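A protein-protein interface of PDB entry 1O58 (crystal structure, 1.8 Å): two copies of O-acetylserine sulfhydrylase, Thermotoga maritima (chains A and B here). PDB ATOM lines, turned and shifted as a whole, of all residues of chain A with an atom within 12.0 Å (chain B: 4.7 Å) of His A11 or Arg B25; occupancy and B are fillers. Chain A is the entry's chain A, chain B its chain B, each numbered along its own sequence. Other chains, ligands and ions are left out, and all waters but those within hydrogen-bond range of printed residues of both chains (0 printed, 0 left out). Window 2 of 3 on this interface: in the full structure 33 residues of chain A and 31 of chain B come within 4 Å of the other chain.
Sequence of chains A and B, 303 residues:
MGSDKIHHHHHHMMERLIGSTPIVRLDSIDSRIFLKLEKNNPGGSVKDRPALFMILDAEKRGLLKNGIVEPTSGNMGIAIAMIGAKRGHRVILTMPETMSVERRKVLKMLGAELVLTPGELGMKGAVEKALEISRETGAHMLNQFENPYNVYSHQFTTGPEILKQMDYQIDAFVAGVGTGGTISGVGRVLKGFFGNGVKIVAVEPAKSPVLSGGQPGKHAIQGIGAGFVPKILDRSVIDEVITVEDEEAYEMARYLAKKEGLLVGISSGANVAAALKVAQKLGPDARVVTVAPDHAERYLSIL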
ATOM      1  N   HIS A  11     -24.036 -12.814   9.745  1.00  0.00           N
ATOM      2  CA  HIS A  11     -23.049 -13.478  10.664  1.00  0.00           C
ATOM      3  C   HIS A  11     -23.611 -14.774  11.252  1.00  0.00           C
ATOM      4  O   HIS A  11     -23.120 -15.262  12.289  1.00  0.00           O
ATOM      5  CB  HIS A  11     -22.599 -12.505  11.779  1.00  0.00           C
ATOM      6  CG  HIS A  11     -21.703 -11.407  11.283  1.00  0.00           C
ATOM      7  ND1 HIS A  11     -22.164 -10.359  10.511  1.00  0.00           N
ATOM      8  CD2 HIS A  11     -20.368 -11.215  11.413  1.00  0.00           C
ATOM      9  CE1 HIS A  11     -21.158  -9.563  10.196  1.00  0.00           C
ATOM     10  NE2 HIS A  11     -20.057 -10.057  10.736  1.00  0.00           N
ATOM     11  N   HIS A  12     -24.631 -15.341  10.592  1.00  0.00           N
ATOM     12  CA  HIS A  12     -25.112 -16.677  10.941  1.00  0.00           C
ATOM     13  C   HIS A  12     -25.623 -16.776  12.376  1.00  0.00           C
ATOM     14  O   HIS A  12     -25.324 -17.746  13.086  1.00  0.00           O
ATOM     15  CB  HIS A  12     -23.977 -17.670  10.707  1.00  0.00           C
ATOM     16  CG  HIS A  12     -23.546 -17.708   9.283  1.00  0.00           C
ATOM     17  ND1 HIS A  12     -22.235 -17.545   8.885  1.00  0.00           N
ATOM     18  CD2 HIS A  12     -24.275 -17.829   8.152  1.00  0.00           C
ATOM     19  CE1 HIS A  12     -22.170 -17.605   7.567  1.00  0.00           C
ATOM     20  NE2 HIS A  12     -23.395 -17.774   7.099  1.00  0.00           N
ATOM     21  N   MET A  13     -26.438 -15.807  12.780  1.00  0.00           N
ATOM     22  CA  MET A  13     -26.892 -15.724  14.175  1.00  0.00           C
ATOM     23  C   MET A  13     -27.569 -16.992  14.660  1.00  0.00           C
ATOM     24  O   MET A  13     -27.164 -17.586  15.656  1.00  0.00           O
ATOM     25  CB  MET A  13     -27.862 -14.550  14.374  1.00  0.00           C
ATOM     26  CG  MET A  13     -28.484 -14.500  15.793  1.00  0.00           C
ATOM     27  SD  MET A  13     -29.576 -13.047  16.064  1.00  0.00           S
ATOM     28  CE  MET A  13     -28.335 -11.834  15.860  1.00  0.00           C
ATOM     29  N   MET A  14     -28.610 -17.397  13.950  1.00  0.00           N
ATOM     30  CA  MET A  14     -29.449 -18.501  14.403  1.00  0.00           C
ATOM     31  C   MET A  14     -28.702 -19.806  14.294  1.00  0.00           C
ATOM     32  O   MET A  14     -28.876 -20.687  15.147  1.00  0.00           O
ATOM     33  CB  MET A  14     -30.767 -18.538  13.619  1.00  0.00           C
ATOM     34  CG  MET A  14     -31.684 -17.346  13.944  1.00  0.00           C
ATOM     35  SD  MET A  14     -32.280 -17.344  15.683  1.00  0.00           S
ATOM     36  CE  MET A  14     -32.894 -15.646  15.714  1.00  0.00           C
ATOM     37  N   GLU A  15     -27.848 -19.908  13.274  1.00  0.00           N
ATOM     38  CA  GLU A  15     -27.042 -21.097  13.053  1.00  0.00           C
ATOM     39  C   GLU A  15     -26.198 -21.346  14.300  1.00  0.00           C
ATOM     40  O   GLU A  15     -26.012 -22.480  14.759  1.00  0.00           O
ATOM     41  CB  GLU A  15     -26.138 -20.929  11.841  1.00  0.00           C
ATOM     42  CG  GLU A  15     -26.862 -20.868  10.487  1.00  0.00           C
ATOM     43  CD  GLU A  15     -27.377 -19.505  10.084  1.00  0.00           C
ATOM     44  OE1 GLU A  15     -27.627 -18.633  10.942  1.00  0.00           O
ATOM     45  OE2 GLU A  15     -27.538 -19.299   8.862  1.00  0.00           O
ATOM     46  N   ARG A  16     -25.624 -20.273  14.824  1.00  0.00           N
ATOM     47  CA  ARG A  16     -24.641 -20.424  15.903  1.00  0.00           C
ATOM     48  C   ARG A  16     -25.289 -20.651  17.252  1.00  0.00           C
ATOM     49  O   ARG A  16     -24.732 -21.340  18.132  1.00  0.00           O
ATOM     50  CB  ARG A  16     -23.741 -19.184  15.933  1.00  0.00           C
ATOM     51  CG  ARG A  16     -22.826 -19.150  14.731  1.00  0.00           C
ATOM     52  CD  ARG A  16     -21.849 -17.970  14.658  1.00  0.00           C
ATOM     53  NE  ARG A  16     -21.087 -17.980  13.400  1.00  0.00           N
ATOM     54  CZ  ARG A  16     -20.159 -17.077  13.064  1.00  0.00           C
ATOM     55  NH1 ARG A  16     -19.875 -16.062  13.872  1.00  0.00           N
ATOM     56  NH2 ARG A  16     -19.509 -17.176  11.900  1.00  0.00           N
ATOM     57  N   LEU A  17     -26.452 -20.052  17.456  1.00  0.00           N
ATOM     58  CA  LEU A  17     -27.151 -20.119  18.717  1.00  0.00           C
ATOM     59  C   LEU A  17     -27.883 -21.428  18.943  1.00  0.00           C
ATOM     60  O   LEU A  17     -28.012 -21.876  20.075  1.00  0.00           O
ATOM     61  CB  LEU A  17     -28.213 -18.993  18.810  1.00  0.00           C
ATOM     62  CG  LEU A  17     -27.703 -17.572  18.984  1.00  0.00           C
ATOM     63  CD1 LEU A  17     -28.847 -16.570  18.868  1.00  0.00           C
ATOM     64  CD2 LEU A  17     -27.014 -17.416  20.321  1.00  0.00           C
ATOM     65  N   ILE A  18     -28.416 -22.013  17.888  1.00  0.00           N
ATOM     66  CA  ILE A  18     -29.265 -23.182  18.035  1.00  0.00           C
ATOM     67  C   ILE A  18     -28.479 -24.462  18.316  1.00  0.00           C
ATOM     68  O   ILE A  18     -27.492 -24.757  17.644  1.00  0.00           O
ATOM     69  CB  ILE A  18     -30.168 -23.304  16.802  1.00  0.00           C
ATOM     70  CG1 ILE A  18     -31.158 -22.126  16.806  1.00  0.00           C
ATOM     71  CG2 ILE A  18     -30.901 -24.602  16.790  1.00  0.00           C
ATOM     72  CD1 ILE A  18     -31.878 -21.971  15.509  1.00  0.00           C
ATOM     73  N   PRO A  42     -32.404 -20.380  21.492  1.00  0.00           N
ATOM     74  CA  PRO A  42     -32.841 -18.977  21.478  1.00  0.00           C
ATOM     75  C   PRO A  42     -34.367 -18.802  21.432  1.00  0.00           C
ATOM     76  O   PRO A  42     -34.912 -17.844  21.983  1.00  0.00           O
ATOM     77  CB  PRO A  42     -32.122 -18.399  20.267  1.00  0.00           C
ATOM     78  CG  PRO A  42     -31.921 -19.601  19.365  1.00  0.00           C
ATOM     79  CD  PRO A  42     -31.561 -20.689  20.319  1.00  0.00           C
ATOM     80  N   LEU A  52     -34.898 -24.624  11.955  1.00  0.00           N
ATOM     81  CA  LEU A  52     -33.736 -24.154  11.220  1.00  0.00           C
ATOM     82  C   LEU A  52     -33.426 -25.068  10.030  1.00  0.00           C
ATOM     83  O   LEU A  52     -33.181 -24.591   8.917  1.00  0.00           O
ATOM     84  CB  LEU A  52     -32.525 -24.060  12.150  1.00  0.00           C
ATOM     85  CG  LEU A  52     -31.225 -23.614  11.464  1.00  0.00           C
ATOM     86  CD1 LEU A  52     -31.292 -22.210  11.001  1.00  0.00           C
ATOM     87  CD2 LEU A  52     -30.007 -23.810  12.387  1.00  0.00           C
ATOM     88  N   LEU A  56     -33.647 -23.794   6.136  1.00  0.00           N
ATOM     89  CA  LEU A  56     -32.431 -23.824   5.329  1.00  0.00           C
ATOM     90  C   LEU A  56     -32.599 -24.645   4.053  1.00  0.00           C
ATOM     91  O   LEU A  56     -32.178 -24.219   2.981  1.00  0.00           O
ATOM     92  CB  LEU A  56     -31.254 -24.339   6.157  1.00  0.00           C
ATOM     93  CG  LEU A  56     -30.787 -23.363   7.250  1.00  0.00           C
ATOM     94  CD1 LEU A  56     -29.607 -23.982   8.002  1.00  0.00           C
ATOM     95  CD2 LEU A  56     -30.431 -22.009   6.659  1.00  0.00           C
ATOM     96  N   GLU A  59     -34.973 -22.570   1.756  1.00  0.00           N
ATOM     97  CA  GLU A  59     -34.224 -21.445   1.185  1.00  0.00           C
ATOM     98  C   GLU A  59     -33.367 -21.865  -0.004  1.00  0.00           C
ATOM     99  O   GLU A  59     -33.419 -21.240  -1.074  1.00  0.00           O
ATOM    100  CB  GLU A  59     -33.332 -20.802   2.231  1.00  0.00           C
ATOM    101  CG  GLU A  59     -34.058 -19.865   3.189  1.00  0.00           C
ATOM    102  CD  GLU A  59     -33.122 -19.271   4.211  1.00  0.00           C
ATOM    103  OE1 GLU A  59     -31.941 -19.700   4.288  1.00  0.00           O
ATOM    104  OE2 GLU A  59     -33.552 -18.364   4.941  1.00  0.00           O
ATOM    105  N   MET A  82     -39.261 -16.819  14.891  1.00  0.00           N
ATOM    106  CA  MET A  82     -37.998 -16.203  15.288  1.00  0.00           C
ATOM    107  C   MET A  82     -37.016 -16.203  14.109  1.00  0.00           C
ATOM    108  O   MET A  82     -36.429 -15.185  13.763  1.00  0.00           O
ATOM    109  CB  MET A  82     -37.384 -17.011  16.441  1.00  0.00           C
ATOM    110  CG  MET A  82     -35.952 -16.655  16.843  1.00  0.00           C
ATOM    111  SD  MET A  82     -35.257 -17.712  18.175  1.00  0.00           S
ATOM    112  CE  MET A  82     -35.119 -19.241  17.257  1.00  0.00           C
ATOM    113  N   ILE A  83     -36.845 -17.361  13.497  1.00  0.00           N
ATOM    114  CA  ILE A  83     -35.899 -17.484  12.365  1.00  0.00           C
ATOM    115  C   ILE A  83     -36.354 -16.644  11.179  1.00  0.00           C
ATOM    116  O   ILE A  83     -35.555 -15.972  10.540  1.00  0.00           O
ATOM    117  CB  ILE A  83     -35.684 -18.961  12.000  1.00  0.00           C
ATOM    118  CG1 ILE A  83     -35.010 -19.686  13.170  1.00  0.00           C
ATOM    119  CG2 ILE A  83     -34.812 -19.069  10.727  1.00  0.00           C
ATOM    120  CD1 ILE A  83     -35.082 -21.185  13.097  1.00  0.00           C
ATOM    121  N   ALA A  85     -38.205 -13.816  11.436  1.00  0.00           N
ATOM    122  CA  ALA A  85     -37.958 -12.434  11.830  1.00  0.00           C
ATOM    123  C   ALA A  85     -36.530 -12.003  11.521  1.00  0.00           C
ATOM    124  O   ALA A  85     -36.310 -10.923  10.954  1.00  0.00           O
ATOM    125  CB  ALA A  85     -38.227 -12.270  13.284  1.00  0.00           C
ATOM    126  N   LYS A  86     -35.570 -12.841  11.895  1.00  0.00           N
ATOM    127  CA  LYS A  86     -34.176 -12.544  11.662  1.00  0.00           C
ATOM    128  C   LYS A  86     -33.824 -12.615  10.177  1.00  0.00           C
ATOM    129  O   LYS A  86     -33.149 -11.716   9.658  1.00  0.00           O
ATOM    130  CB  LYS A  86     -33.264 -13.483  12.479  1.00  0.00           C
ATOM    131  CG  LYS A  86     -31.758 -13.282  12.215  1.00  0.00           C
ATOM    132  CD  LYS A  86     -31.300 -11.838  12.411  1.00  0.00           C
ATOM    133  CE  LYS A  86     -29.785 -11.717  12.359  1.00  0.00           C
ATOM    134  NZ  LYS A  86     -29.327 -10.269  12.347  1.00  0.00           N
ATOM    135  N   ARG A  87     -34.300 -13.658   9.495  1.00  0.00           N
ATOM    136  CA  ARG A  87     -33.860 -13.951   8.120  1.00  0.00           C
ATOM    137  C   ARG A  87     -34.713 -13.324   7.016  1.00  0.00           C
ATOM    138  O   ARG A  87     -34.378 -13.425   5.840  1.00  0.00           O
ATOM    139  CB  ARG A  87     -33.746 -15.480   7.886  1.00  0.00           C
ATOM    140  CG  ARG A  87     -32.756 -16.181   8.775  1.00  0.00           C
ATOM    141  CD  ARG A  87     -32.693 -17.691   8.501  1.00  0.00           C
ATOM    142  NE  ARG A  87     -31.969 -18.022   7.280  1.00  0.00           N
ATOM    143  CZ  ARG A  87     -30.648 -18.151   7.220  1.00  0.00           C
ATOM    144  NH1 ARG A  87     -29.899 -17.879   8.281  1.00  0.00           N
ATOM    145  NH2 ARG A  87     -30.068 -18.467   6.085  1.00  0.00           N
ATOM    146  N   ILE B  23     -22.682 -14.644  22.658  1.00  0.00           N
ATOM    147  CA  ILE B  23     -22.786 -13.268  22.210  1.00  0.00           C
ATOM    148  C   ILE B  23     -23.198 -13.287  20.739  1.00  0.00           C
ATOM    149  O   ILE B  23     -22.706 -14.118  19.957  1.00  0.00           O
ATOM    150  CB  ILE B  23     -21.454 -12.499  22.371  1.00  0.00           C
ATOM    151  CG1 ILE B  23     -21.108 -12.338  23.834  1.00  0.00           C
ATOM    152  CG2 ILE B  23     -21.543 -11.142  21.709  1.00  0.00           C
ATOM    153  CD1 ILE B  23     -19.801 -11.569  24.060  1.00  0.00           C
ATOM    154  N   VAL B  24     -24.122 -12.416  20.401  1.00  0.00           N
ATOM    155  CA  VAL B  24     -24.612 -12.252  19.026  1.00  0.00           C
ATOM    156  C   VAL B  24     -24.408 -10.831  18.571  1.00  0.00           C
ATOM    157  O   VAL B  24     -24.567  -9.918  19.351  1.00  0.00           O
ATOM    158  CB  VAL B  24     -26.128 -12.576  18.913  1.00  0.00           C
ATOM    159  CG1 VAL B  24     -26.358 -14.012  19.191  1.00  0.00           C
ATOM    160  CG2 VAL B  24     -26.961 -11.736  19.858  1.00  0.00           C
ATOM    161  N   ARG B  25     -24.084 -10.648  17.298  1.00  0.00           N
ATOM    162  CA  ARG B  25     -23.926  -9.328  16.691  1.00  0.00           C
ATOM    163  C   ARG B  25     -25.263  -8.871  16.127  1.00  0.00           C
ATOM    164  O   ARG B  25     -25.954  -9.642  15.427  1.00  0.00           O
ATOM    165  CB  ARG B  25     -22.913  -9.435  15.562  1.00  0.00           C
ATOM    166  CG  ARG B  25     -22.569  -8.147  14.883  1.00  0.00           C
ATOM    167  CD  ARG B  25     -21.446  -8.394  13.858  1.00  0.00           C
ATOM    168  NE  ARG B  25     -20.717  -7.180  13.567  1.00  0.00           N
ATOM    169  CZ  ARG B  25     -19.451  -7.164  13.189  1.00  0.00           C
ATOM    170  NH1 ARG B  25     -18.757  -8.297  13.044  1.00  0.00           N
ATOM    171  NH2 ARG B  25     -18.879  -5.997  12.958  1.00  0.00           N
ATOM    172  N   LEU B  26     -25.652  -7.631  16.412  1.00  0.00           N
ATOM    173  CA  LEU B  26     -27.009  -7.174  16.066  1.00  0.00           C
ATOM    174  C   LEU B  26     -27.066  -6.582  14.648  1.00  0.00           C
ATOM    175  O   LEU B  26     -27.322  -5.397  14.488  1.00  0.00           O
ATOM    176  CB  LEU B  26     -27.516  -6.167  17.096  1.00  0.00           C
ATOM    177  CG  LEU B  26     -27.522  -6.704  18.532  1.00  0.00           C
ATOM    178  CD1 LEU B  26     -28.110  -5.651  19.485  1.00  0.00           C
ATOM    179  CD2 LEU B  26     -28.325  -8.000  18.613  1.00  0.00           C
ATOM    180  N   ASP B  27     -26.829  -7.440  13.652  1.00  0.00           N
ATOM    181  CA  ASP B  27     -26.692  -7.010  12.249  1.00  0.00           C
ATOM    182  C   ASP B  27     -27.931  -6.384  11.660  1.00  0.00           C
ATOM    183  O   ASP B  27     -27.822  -5.583  10.712  1.00  0.00           O
ATOM    184  CB  ASP B  27     -26.287  -8.162  11.349  1.00  0.00           C
ATOM    185  CG  ASP B  27     -24.872  -8.485  11.453  1.00  0.00           C
ATOM    186  OD1 ASP B  27     -24.073  -7.531  11.491  1.00  0.00           O
ATOM    187  OD2 ASP B  27     -24.454  -9.666  11.504  1.00  0.00           O
ATOM    188  N   SER B  31     -24.599  -3.345  13.244  1.00  0.00           N
ATOM    189  CA  SER B  31     -23.580  -4.398  13.331  1.00  0.00           C
ATOM    190  C   SER B  31     -22.381  -4.094  14.273  1.00  0.00           C
ATOM    191  O   SER B  31     -21.514  -4.966  14.506  1.00  0.00           O
ATOM    192  CB  SER B  31     -23.071  -4.700  11.921  1.00  0.00           C
ATOM    193  OG  SER B  31     -22.399  -3.575  11.420  1.00  0.00           O
ATOM    194  N   ILE B  33     -22.926  -3.449  17.430  1.00  0.00           N
ATOM    195  CA  ILE B  33     -23.384  -3.863  18.767  1.00  0.00           C
ATOM    196  C   ILE B  33     -23.387  -5.386  18.910  1.00  0.00           C
ATOM    197  O   ILE B  33     -23.932  -6.087  18.070  1.00  0.00           O
ATOM    198  CB  ILE B  33     -24.809  -3.291  19.079  1.00  0.00           C
ATOM    199  CG1 ILE B  33     -24.856  -1.774  18.915  1.00  0.00           C
ATOM    200  CG2 ILE B  33     -25.197  -3.672  20.508  1.00  0.00           C
ATOM    201  CD1 ILE B  33     -26.289  -1.232  19.026  1.00  0.00           C
ATOM    202  N   PHE B  34     -22.797  -5.878  19.999  1.00  0.00           N
ATOM    203  CA  PHE B  34     -22.695  -7.282  20.303  1.00  0.00           C
ATOM    204  C   PHE B  34     -23.397  -7.479  21.624  1.00  0.00           C
ATOM    205  O   PHE B  34     -23.121  -6.762  22.593  1.00  0.00           O
ATOM    206  CB  PHE B  34     -21.231  -7.669  20.440  1.00  0.00           C
ATOM    207  CG  PHE B  34     -20.458  -7.532  19.162  1.00  0.00           C
ATOM    208  CD1 PHE B  34     -20.121  -6.293  18.685  1.00  0.00           C
ATOM    209  CD2 PHE B  34     -20.114  -8.650  18.436  1.00  0.00           C
ATOM    210  CE1 PHE B  34     -19.412  -6.155  17.464  1.00  0.00           C
ATOM    211  CE2 PHE B  34     -19.390  -8.532  17.217  1.00  0.00           C
ATOM    212  CZ  PHE B  34     -19.047  -7.290  16.755  1.00  0.00           C
ATOM    213  N   GLU B 260     -34.533  -8.879  15.265  1.00  0.00           N
ATOM    214  CA  GLU B 260     -33.458  -9.849  15.475  1.00  0.00           C
ATOM    215  C   GLU B 260     -33.966 -11.223  15.915  1.00  0.00           C
ATOM    216  O   GLU B 260     -33.196 -12.171  15.953  1.00  0.00           O
ATOM    217  CB  GLU B 260     -32.439  -9.333  16.500  1.00  0.00           C
ATOM    218  CG  GLU B 260     -31.741  -8.046  16.065  1.00  0.00           C
ATOM    219  CD  GLU B 260     -30.630  -8.264  15.045  1.00  0.00           C
ATOM    220  OE1 GLU B 260     -30.017  -7.247  14.639  1.00  0.00           O
ATOM    221  OE2 GLU B 260     -30.374  -9.425  14.663  1.00  0.00           O
ATOM    222  N   ARG B 287     -16.581  -1.667  18.097  1.00  0.00           N
ATOM    223  CA  ARG B 287     -17.145  -2.890  18.622  1.00  0.00           C
ATOM    224  C   ARG B 287     -17.625  -2.574  20.020  1.00  0.00           C
ATOM    225  O   ARG B 287     -16.816  -2.292  20.904  1.00  0.00           O
ATOM    226  CB  ARG B 287     -16.119  -4.008  18.614  1.00  0.00           C
ATOM    227  CG  ARG B 287     -15.711  -4.398  17.173  1.00  0.00           C
ATOM    228  CD  ARG B 287     -14.419  -5.204  17.044  1.00  0.00           C
ATOM    229  NE  ARG B 287     -14.424  -6.472  17.760  1.00  0.00           N
ATOM    230  CZ  ARG B 287     -14.908  -7.627  17.312  1.00  0.00           C
ATOM    231  NH1 ARG B 287     -15.485  -7.729  16.129  1.00  0.00           N
ATOM    232  NH2 ARG B 287     -14.792  -8.706  18.055  1.00  0.00           N
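NE2 of His A11 is in hydrogen-bond range of NH1 of Arg B25.
A ring nitrogen (ND1) of His A11 sits at hydrogen-bond distance from the side-chain carboxylate (OD2) of Asp B27 (2.6 Å).
NZ of Lys A86 lies within salt-bridge range of OE2 of Glu B260, 2.7 Å away.
The side-chain sulfur of Met A13 sits close to the backbone carbonyl oxygen of Glu B260, at 3.7 Å.
The guanidinium group of Arg B25 lies within salt-bridge range of the side-chain carboxylate of Asp B27, 3.96 Å away.
The backbone carbonyl oxygen of Ser B31 lies within hydrogen-bond range of the guanidinium group of Arg B25.
The backbone NH (N) of Asp B27 lies within hydrogen-bond range of the side-chain carboxylate (OE1) of Glu B260 (3.3 Å).
Among the printed residues, merely in contact across the chains: Met A13 with Val B24, Met A13 with Arg B25, Met A14 with Glu B260, Leu A17 with Val B24 and Lys A86 with Asp B27.
Of chain B, only Arg B25 and Asp B27 come within 4 Å of His A11.
Arg B25 touches just these residues of chain A: His A11 and Met A13.
Val B24 touches two residues of chain A.
Leu B26 touches none of the printed residues of chain A.
Of chain A, only His A11 (2.6 Å) and Lys A86 (3.8 Å) come within 4 Å of Asp B27.
No residue of chain A comes within 4 Å of Phe B34.
Of the printed residues of chain B, Leu A17 touches Val B24.
Printed residues of chain A within 4 Å of Glu B260: Met A13 (3.4 Å), Met A14 (3.5 Å) and Lys A86 (2.7 Å).
Of the printed residues of chain B, Lys A86 touches Asp B27 (3.8 Å) and Glu B260 (2.7 Å).
Of the printed residues of chain B, Met A14 touches Glu B260 (3.5 Å).
Pro A42 touches none of the printed residues of chain B.
The nearest printed residue of chain B that does not touch His A11 is Ser B31 (5.5 Å).
The nearest residue of chain A that does not touch Arg B25 is Lys A86 (4.6 Å).
Hydrophobic or aromatic side chains of chain B within 4 Å of the printed part of chain A: Val B24.
Along chain B the printed residues that touch a printed residue of chain A span positions 24 to 260.
Printed residues of chain A that touch a printed residue of chain B: His A11, Met A13, Met A14, Leu A17 and Lys A86.
Among the printed residues, 9 pairs touch across the chains.
Among the printed residues, Asp or Glu carboxylates within 4 Å of a Lys or Arg side-chain nitrogen of the other chain: Lys A86 with Glu B260.
No position is printed for both chains.
Of the 9 pairs that touch across the chains among the printed residues, none has its exchanged pair printed and touching as well.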
